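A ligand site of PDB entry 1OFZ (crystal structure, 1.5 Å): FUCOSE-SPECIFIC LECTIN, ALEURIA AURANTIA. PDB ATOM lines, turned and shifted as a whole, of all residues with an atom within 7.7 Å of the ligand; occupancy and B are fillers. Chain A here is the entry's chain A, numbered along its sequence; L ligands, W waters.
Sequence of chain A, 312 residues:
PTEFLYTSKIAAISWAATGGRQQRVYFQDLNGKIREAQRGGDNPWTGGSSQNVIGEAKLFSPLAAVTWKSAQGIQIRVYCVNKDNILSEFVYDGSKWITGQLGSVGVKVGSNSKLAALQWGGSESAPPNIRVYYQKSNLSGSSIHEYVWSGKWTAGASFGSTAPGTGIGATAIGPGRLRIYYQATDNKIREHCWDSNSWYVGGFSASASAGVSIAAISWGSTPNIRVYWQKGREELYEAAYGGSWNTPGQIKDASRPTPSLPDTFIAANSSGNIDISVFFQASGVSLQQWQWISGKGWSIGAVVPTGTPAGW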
ATOM      1  N   ILE A  13      24.671  15.599  17.952  1.00  0.00           N
ATOM      2  CA  ILE A  13      25.833  16.067  17.205  1.00  0.00           C
ATOM      3  C   ILE A  13      26.858  14.930  17.124  1.00  0.00           C
ATOM      4  O   ILE A  13      26.804  13.973  17.889  1.00  0.00           O
ATOM      5  CB  ILE A  13      26.469  17.293  17.882  1.00  0.00           C
ATOM      6  CG1 ILE A  13      26.897  16.972  19.348  1.00  0.00           C
ATOM      7  CG2 ILE A  13      25.507  18.492  17.799  1.00  0.00           C
ATOM      8  CD1 ILE A  13      27.570  18.092  20.063  1.00  0.00           C
ATOM      9  N   TRP A  15      31.235  14.264  15.689  1.00  0.00           N
ATOM     10  CA  TRP A  15      32.445  14.715  15.011  1.00  0.00           C
ATOM     11  C   TRP A  15      33.450  13.570  14.928  1.00  0.00           C
ATOM     12  O   TRP A  15      33.431  12.663  15.733  1.00  0.00           O
ATOM     13  CB  TRP A  15      33.065  15.944  15.641  1.00  0.00           C
ATOM     14  CG  TRP A  15      33.526  15.800  17.055  1.00  0.00           C
ATOM     15  CD1 TRP A  15      34.802  15.542  17.468  1.00  0.00           C
ATOM     16  CD2 TRP A  15      32.741  15.926  18.239  1.00  0.00           C
ATOM     17  NE1 TRP A  15      34.854  15.490  18.835  1.00  0.00           N
ATOM     18  CE2 TRP A  15      33.602  15.694  19.345  1.00  0.00           C
ATOM     19  CE3 TRP A  15      31.385  16.133  18.490  1.00  0.00           C
ATOM     20  CZ2 TRP A  15      33.160  15.728  20.680  1.00  0.00           C
ATOM     21  CZ3 TRP A  15      30.951  16.185  19.815  1.00  0.00           C
ATOM     22  CH2 TRP A  15      31.835  15.979  20.885  1.00  0.00           C
ATOM     23  N   GLN A  22      32.991  10.799  17.841  1.00  0.00           N
ATOM     24  CA  GLN A  22      32.416  11.236  19.106  1.00  0.00           C
ATOM     25  C   GLN A  22      31.013  11.693  18.812  1.00  0.00           C
ATOM     26  O   GLN A  22      30.831  12.427  17.867  1.00  0.00           O
ATOM     27  CB  GLN A  22      33.224  12.373  19.677  1.00  0.00           C
ATOM     28  CG  GLN A  22      34.565  11.949  20.284  1.00  0.00           C
ATOM     29  CD  GLN A  22      34.420  11.123  21.526  1.00  0.00           C
ATOM     30  OE1 GLN A  22      33.533  11.344  22.360  1.00  0.00           O
ATOM     31  NE2 GLN A  22      35.363  10.162  21.699  1.00  0.00           N
ATOM     32  N   GLN A  23      30.068  11.246  19.620  1.00  0.00           N
ATOM     33  CA  GLN A  23      28.676  11.678  19.529  1.00  0.00           C
ATOM     34  C   GLN A  23      28.233  12.256  20.829  1.00  0.00           C
ATOM     35  O   GLN A  23      28.630  11.799  21.907  1.00  0.00           O
ATOM     36  CB  GLN A  23      27.775  10.512  19.216  1.00  0.00           C
ATOM     37  CG  GLN A  23      28.041   9.824  17.907  1.00  0.00           C
ATOM     38  CD  GLN A  23      27.042   8.754  17.643  1.00  0.00           C
ATOM     39  OE1 GLN A  23      25.841   9.010  17.387  1.00  0.00           O
ATOM     40  NE2 GLN A  23      27.479   7.516  17.771  1.00  0.00           N
ATOM     41  N   ARG A  24      27.335  13.224  20.783  1.00  0.00           N
ATOM     42  CA  ARG A  24      26.646  13.689  21.973  1.00  0.00           C
ATOM     43  C   ARG A  24      25.178  13.756  21.631  1.00  0.00           C
ATOM     44  O   ARG A  24      24.814  14.175  20.502  1.00  0.00           O
ATOM     45  CB  ARG A  24      27.095  15.063  22.450  1.00  0.00           C
ATOM     46  CG  ARG A  24      28.596  15.201  22.682  1.00  0.00           C
ATOM     47  CD  ARG A  24      29.074  14.365  23.922  1.00  0.00           C
ATOM     48  NE  ARG A  24      30.496  14.560  24.200  1.00  0.00           N
ATOM     49  CZ  ARG A  24      31.467  13.806  23.680  1.00  0.00           C
ATOM     50  NH1 ARG A  24      31.217  12.802  22.891  1.00  0.00           N
ATOM     51  NH2 ARG A  24      32.734  14.091  23.979  1.00  0.00           N
ATOM     52  N   VAL A  25      24.335  13.397  22.592  1.00  0.00           N
ATOM     53  CA  VAL A  25      22.906  13.511  22.435  1.00  0.00           C
ATOM     54  C   VAL A  25      22.330  14.180  23.648  1.00  0.00           C
ATOM     55  O   VAL A  25      22.778  13.937  24.756  1.00  0.00           O
ATOM     56  CB  VAL A  25      22.237  12.148  22.130  1.00  0.00           C
ATOM     57  CG1 VAL A  25      22.435  11.121  23.228  1.00  0.00           C
ATOM     58  CG2 VAL A  25      20.767  12.324  21.783  1.00  0.00           C
ATOM     59  N   TYR A  26      21.336  15.054  23.403  1.00  0.00           N
ATOM     60  CA  TYR A  26      20.708  15.906  24.425  1.00  0.00           C
ATOM     61  C   TYR A  26      19.225  15.600  24.502  1.00  0.00           C
ATOM     62  O   TYR A  26      18.568  15.452  23.461  1.00  0.00           O
ATOM     63  CB  TYR A  26      20.914  17.424  24.118  1.00  0.00           C
ATOM     64  CG  TYR A  26      22.376  17.728  24.010  1.00  0.00           C
ATOM     65  CD1 TYR A  26      23.144  17.912  25.168  1.00  0.00           C
ATOM     66  CD2 TYR A  26      23.047  17.660  22.795  1.00  0.00           C
ATOM     67  CE1 TYR A  26      24.503  18.078  25.084  1.00  0.00           C
ATOM     68  CE2 TYR A  26      24.401  17.843  22.697  1.00  0.00           C
ATOM     69  CZ  TYR A  26      25.138  17.990  23.871  1.00  0.00           C
ATOM     70  OH  TYR A  26      26.510  18.093  23.786  1.00  0.00           O
ATOM     71  N   GLU A  36      23.019  15.253  28.839  1.00  0.00           N
ATOM     72  CA  GLU A  36      23.858  14.810  27.763  1.00  0.00           C
ATOM     73  C   GLU A  36      24.258  13.372  27.959  1.00  0.00           C
ATOM     74  O   GLU A  36      24.600  12.963  29.086  1.00  0.00           O
ATOM     75  CB  GLU A  36      25.132  15.659  27.733  1.00  0.00           C
ATOM     76  CG  GLU A  36      26.057  15.379  26.557  1.00  0.00           C
ATOM     77  CD  GLU A  36      27.384  16.084  26.700  1.00  0.00           C
ATOM     78  OE1 GLU A  36      28.139  15.731  27.677  1.00  0.00           O
ATOM     79  OE2 GLU A  36      27.704  16.980  25.908  1.00  0.00           O
ATOM     80  N   ALA A  37      24.266  12.615  26.877  1.00  0.00           N
ATOM     81  CA  ALA A  37      24.905  11.290  26.820  1.00  0.00           C
ATOM     82  C   ALA A  37      25.954  11.360  25.730  1.00  0.00           C
ATOM     83  O   ALA A  37      25.871  12.186  24.793  1.00  0.00           O
ATOM     84  CB  ALA A  37      23.933  10.223  26.564  1.00  0.00           C
ATOM     85  N   GLN A  38      26.985  10.528  25.854  1.00  0.00           N
ATOM     86  CA  GLN A  38      28.159  10.596  25.003  1.00  0.00           C
ATOM     87  C   GLN A  38      28.520   9.225  24.455  1.00  0.00           C
ATOM     88  O   GLN A  38      28.271   8.189  25.104  1.00  0.00           O
ATOM     89  CB  GLN A  38      29.338  11.105  25.790  1.00  0.00           C
ATOM     90  CG  GLN A  38      29.110  12.284  26.692  1.00  0.00           C
ATOM     91  CD  GLN A  38      28.575  11.991  28.077  1.00  0.00           C
ATOM     92  OE1 GLN A  38      28.720  10.840  28.603  1.00  0.00           O
ATOM     93  NE2 GLN A  38      28.001  12.999  28.721  1.00  0.00           N
ATOM     94  N   THR A  46      27.720   6.495  27.306  1.00  0.00           N
ATOM     95  CA  THR A  46      27.902   6.955  28.658  1.00  0.00           C
ATOM     96  C   THR A  46      27.043   8.146  28.965  1.00  0.00           C
ATOM     97  O   THR A  46      26.396   8.715  28.077  1.00  0.00           O
ATOM     98  CB  THR A  46      29.376   7.334  28.872  1.00  0.00           C
ATOM     99  OG1 THR A  46      29.769   8.410  27.988  1.00  0.00           O
ATOM    100  CG2 THR A  46      30.338   6.182  28.522  1.00  0.00           C
ATOM    101  N   ASN A  52      24.881  14.493  34.507  1.00  0.00           N
ATOM    102  CA  ASN A  52      25.156  14.913  33.131  1.00  0.00           C
ATOM    103  C   ASN A  52      24.234  16.018  32.707  1.00  0.00           C
ATOM    104  O   ASN A  52      23.892  16.107  31.542  1.00  0.00           O
ATOM    105  CB  ASN A  52      25.060  13.736  32.201  1.00  0.00           C
ATOM    106  CG  ASN A  52      26.044  12.648  32.558  1.00  0.00           C
ATOM    107  OD1 ASN A  52      25.655  11.631  33.067  1.00  0.00           O
ATOM    108  ND2 ASN A  52      27.333  12.891  32.277  1.00  0.00           N
ATOM    109  N   VAL A  53      23.813  16.837  33.634  1.00  0.00           N
ATOM    110  CA  VAL A  53      22.949  17.984  33.303  1.00  0.00           C
ATOM    111  C   VAL A  53      23.769  19.134  32.711  1.00  0.00           C
ATOM    112  O   VAL A  53      24.815  19.546  33.301  1.00  0.00           O
ATOM    113  CB  VAL A  53      22.181  18.466  34.557  1.00  0.00           C
ATOM    114  CG1 VAL A  53      21.539  19.833  34.300  1.00  0.00           C
ATOM    115  CG2 VAL A  53      21.177  17.417  35.009  1.00  0.00           C
ATOM    116  N   ILE A  54      23.333  19.673  31.559  1.00  0.00           N
ATOM    117  CA  ILE A  54      24.040  20.771  30.888  1.00  0.00           C
ATOM    118  C   ILE A  54      23.270  22.089  30.891  1.00  0.00           C
ATOM    119  O   ILE A  54      23.827  23.142  30.559  1.00  0.00           O
ATOM    120  CB  ILE A  54      24.468  20.381  29.446  1.00  0.00           C
ATOM    121  CG1 ILE A  54      23.271  20.153  28.515  1.00  0.00           C
ATOM    122  CG2 ILE A  54      25.321  19.130  29.463  1.00  0.00           C
ATOM    123  CD1 ILE A  54      22.826  21.387  27.769  1.00  0.00           C
ATOM    124  N   THR A  67      27.862  21.921  16.735  1.00  0.00           N
ATOM    125  CA  THR A  67      29.204  21.792  17.258  1.00  0.00           C
ATOM    126  C   THR A  67      30.223  22.137  16.151  1.00  0.00           C
ATOM    127  O   THR A  67      29.974  21.986  14.949  1.00  0.00           O
ATOM    128  CB  THR A  67      29.418  20.358  17.770  1.00  0.00           C
ATOM    129  OG1 THR A  67      30.703  20.260  18.429  1.00  0.00           O
ATOM    130  CG2 THR A  67      29.468  19.379  16.672  1.00  0.00           C
ATOM    131  N   GLY A  73      39.110  23.992  22.104  1.00  0.00           N
ATOM    132  CA  GLY A  73      38.497  22.675  22.235  1.00  0.00           C
ATOM    133  C   GLY A  73      37.179  22.600  21.496  1.00  0.00           C
ATOM    134  O   GLY A  73      36.847  23.450  20.671  1.00  0.00           O
ATOM    135  N   ILE A  74      36.433  21.569  21.810  1.00  0.00           N
ATOM    136  CA  ILE A  74      35.160  21.337  21.175  1.00  0.00           C
ATOM    137  C   ILE A  74      34.129  22.369  21.678  1.00  0.00           C
ATOM    138  O   ILE A  74      33.965  22.573  22.885  1.00  0.00           O
ATOM    139  CB  ILE A  74      34.678  19.914  21.481  1.00  0.00           C
ATOM    140  CG1 ILE A  74      35.696  18.886  20.996  1.00  0.00           C
ATOM    141  CG2 ILE A  74      33.297  19.665  20.845  1.00  0.00           C
ATOM    142  CD1 ILE A  74      35.994  18.844  19.603  1.00  0.00           C
ATOM    143  N   GLN A  75      33.480  23.047  20.735  1.00  0.00           N
ATOM    144  CA  GLN A  75      32.437  23.999  20.996  1.00  0.00           C
ATOM    145  C   GLN A  75      31.085  23.323  20.718  1.00  0.00           C
ATOM    146  O   GLN A  75      30.937  22.645  19.716  1.00  0.00           O
ATOM    147  CB  GLN A  75      32.573  25.217  20.083  1.00  0.00           C
ATOM    148  CG  GLN A  75      33.804  26.025  20.298  1.00  0.00           C
ATOM    149  CD  GLN A  75      33.848  26.796  21.607  1.00  0.00           C
ATOM    150  OE1 GLN A  75      32.846  27.159  22.194  1.00  0.00           O
ATOM    151  NE2 GLN A  75      35.062  27.083  22.065  1.00  0.00           N
ATOM    152  N   ILE A  76      30.170  23.427  21.665  1.00  0.00           N
ATOM    153  CA  ILE A  76      28.789  22.937  21.526  1.00  0.00           C
ATOM    154  C   ILE A  76      27.860  24.052  21.877  1.00  0.00           C
ATOM    155  O   ILE A  76      28.090  24.784  22.856  1.00  0.00           O
ATOM    156  CB  ILE A  76      28.499  21.679  22.399  1.00  0.00           C
ATOM    157  CG1 ILE A  76      29.545  20.634  22.104  1.00  0.00           C
ATOM    158  CG2 ILE A  76      27.082  21.166  22.109  1.00  0.00           C
ATOM    159  CD1 ILE A  76      29.513  19.443  23.033  1.00  0.00           C
ATOM    160  N   TYR A  92      28.903  24.884  25.595  1.00  0.00           N
ATOM    161  CA  TYR A  92      30.114  24.203  26.048  1.00  0.00           C
ATOM    162  C   TYR A  92      31.234  24.923  25.361  1.00  0.00           C
ATOM    163  O   TYR A  92      31.342  24.893  24.109  1.00  0.00           O
ATOM    164  CB  TYR A  92      30.144  22.750  25.659  1.00  0.00           C
ATOM    165  CG  TYR A  92      31.297  22.018  26.281  1.00  0.00           C
ATOM    166  CD1 TYR A  92      31.309  21.702  27.646  1.00  0.00           C
ATOM    167  CD2 TYR A  92      32.407  21.675  25.513  1.00  0.00           C
ATOM    168  CE1 TYR A  92      32.399  21.010  28.217  1.00  0.00           C
ATOM    169  CE2 TYR A  92      33.497  20.982  26.083  1.00  0.00           C
ATOM    170  CZ  TYR A  92      33.465  20.690  27.416  1.00  0.00           C
ATOM    171  OH  TYR A  92      34.555  20.004  27.957  1.00  0.00           O
ATOM    172  N   GLY A  94      34.543  24.473  25.315  1.00  0.00           N
ATOM    173  CA  GLY A  94      35.742  23.690  25.220  1.00  0.00           C
ATOM    174  C   GLY A  94      36.155  23.075  26.534  1.00  0.00           C
ATOM    175  O   GLY A  94      36.972  22.140  26.540  1.00  0.00           O
ATOM    176  N   SER A  95      35.631  23.591  27.644  1.00  0.00           N
ATOM    177  CA  SER A  95      35.975  23.022  28.952  1.00  0.00           C
ATOM    178  C   SER A  95      34.826  22.930  29.958  1.00  0.00           C
ATOM    179  O   SER A  95      34.887  22.119  30.863  1.00  0.00           O
ATOM    180  CB  SER A  95      37.151  23.784  29.554  1.00  0.00           C
ATOM    181  OG  SER A  95      36.773  25.092  29.898  1.00  0.00           O
ATOM    182  N   LYS A  96      33.789  23.743  29.807  1.00  0.00           N
ATOM    183  CA  LYS A  96      32.682  23.770  30.754  1.00  0.00           C
ATOM    184  C   LYS A  96      31.384  24.249  30.083  1.00  0.00           C
ATOM    185  O   LYS A  96      31.408  24.898  29.016  1.00  0.00           O
ATOM    186  CB  LYS A  96      33.006  24.700  31.906  1.00  0.00           C
ATOM    187  CG  LYS A  96      33.198  26.140  31.496  1.00  0.00           C
ATOM    188  CD  LYS A  96      33.612  27.033  32.708  1.00  0.00           C
ATOM    189  CE  LYS A  96      33.851  28.443  32.273  1.00  0.00           C
ATOM    190  NZ  LYS A  96      34.972  28.591  31.345  1.00  0.00           N
ATOM    191  N   TRP A  97      30.266  23.964  30.738  1.00  0.00           N
ATOM    192  CA  TRP A  97      28.934  24.391  30.312  1.00  0.00           C
ATOM    193  C   TRP A  97      28.545  25.691  31.030  1.00  0.00           C
ATOM    194  O   TRP A  97      28.644  25.782  32.285  1.00  0.00           O
ATOM    195  CB  TRP A  97      27.911  23.303  30.631  1.00  0.00           C
ATOM    196  CG  TRP A  97      28.007  22.134  29.726  1.00  0.00           C
ATOM    197  CD1 TRP A  97      28.670  20.984  29.961  1.00  0.00           C
ATOM    198  CD2 TRP A  97      27.465  22.028  28.399  1.00  0.00           C
ATOM    199  NE1 TRP A  97      28.587  20.154  28.862  1.00  0.00           N
ATOM    200  CE2 TRP A  97      27.831  20.774  27.896  1.00  0.00           C
ATOM    201  CE3 TRP A  97      26.705  22.882  27.572  1.00  0.00           C
ATOM    202  CZ2 TRP A  97      27.456  20.325  26.621  1.00  0.00           C
ATOM    203  CZ3 TRP A  97      26.315  22.450  26.344  1.00  0.00           C
ATOM    204  CH2 TRP A  97      26.684  21.185  25.863  1.00  0.00           C
HETATM  205  C1  LIG L   1      33.234  15.916  27.387  1.00  0.00           C
HETATM  206  C2  LIG L   1      31.824  16.042  27.961  1.00  0.00           C
HETATM  207  O1  LIG L   1      31.914  15.763  29.379  1.00  0.00           O
HETATM  208  C3  LIG L   1      31.265  17.435  27.741  1.00  0.00           C
HETATM  209  O2  LIG L   1      29.972  17.555  28.323  1.00  0.00           O
HETATM  210  C4  LIG L   1      31.263  17.762  26.256  1.00  0.00           C
HETATM  211  O3  LIG L   1      30.334  17.006  25.533  1.00  0.00           O
HETATM  212  C5  LIG L   1      32.690  17.534  25.761  1.00  0.00           C
HETATM  213  C6  LIG L   1      32.822  17.898  24.285  1.00  0.00           C
HETATM  214  O4  LIG L   1      32.995  16.146  25.965  1.00  0.00           O
HETATM  215  O5  LIG L   1      33.697  14.580  27.351  1.00  0.00           O
HETATM  216  O   HOH W   1      36.241  15.275  26.549  1.00  0.00           O
HETATM  217  O   HOH W   2      34.266  16.330  30.723  1.00  0.00           O
HETATM  218  O   HOH W   3      32.451  12.167  26.932  1.00  0.00           O
HETATM  219  O   HOH W   4      36.815  13.125  27.633  1.00  0.00           O
HETATM  220  O   HOH W   5      30.253  17.965  31.213  1.00  0.00           O
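An oxygen (O3) of the ligand is in hydrogen-bond range of the side-chain carboxylate (OE2) of Glu 36, 2.7 Å away.
An oxygen (O3) of the ligand sits at hydrogen-bond distance from the guanidinium group (NE) of Arg 24.
An oxygen (O2) of the ligand sits at hydrogen-bond distance from the indole nitrogen (NE1) of Trp 97 (3.0 Å).
The backbone carbonyl oxygen (O) of Arg 24 is in hydrogen-bond range of the backbone NH (N) of Ile 13 (2.9 Å).
OH of Tyr 26 sits at hydrogen-bond distance from OE2 of Glu 36, at 2.7 Å.
The side-chain carboxylate (OE1) of Glu 36 is in hydrogen-bond range of the side-chain amide nitrogen (NE2) of Gln 38 (2.9 Å).
NH1 of Arg 24 lies within hydrogen-bond range of OE1 of Gln 22, 2.8 Å away.
The backbone carbonyl oxygen of Asn 52 lies within hydrogen-bond range of the backbone NH of Glu 36, at 3.0 Å.
The backbone carbonyl oxygen (O) of Ile 74 is in hydrogen-bond range of the backbone NH (N) of Gly 94, 3.1 Å away.
The backbone NH (N) of Tyr 92 lies within hydrogen-bond range of the backbone carbonyl oxygen (O) of Ile 76, 2.9 Å away.
OE1 of Gln 75 lies close to O of Tyr 92 (3.3 Å).
Ile 74 touches the ligand.
Ile 76 touches the ligand (CD1 to O3, 3.6 Å).
Tyr 92 touches the ligand (CE2 to C5, 3.6 Å).
Hydrophobic or aromatic side chains that line the ligand: Ile 74, Ile 76, Tyr 92 and Trp 97.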
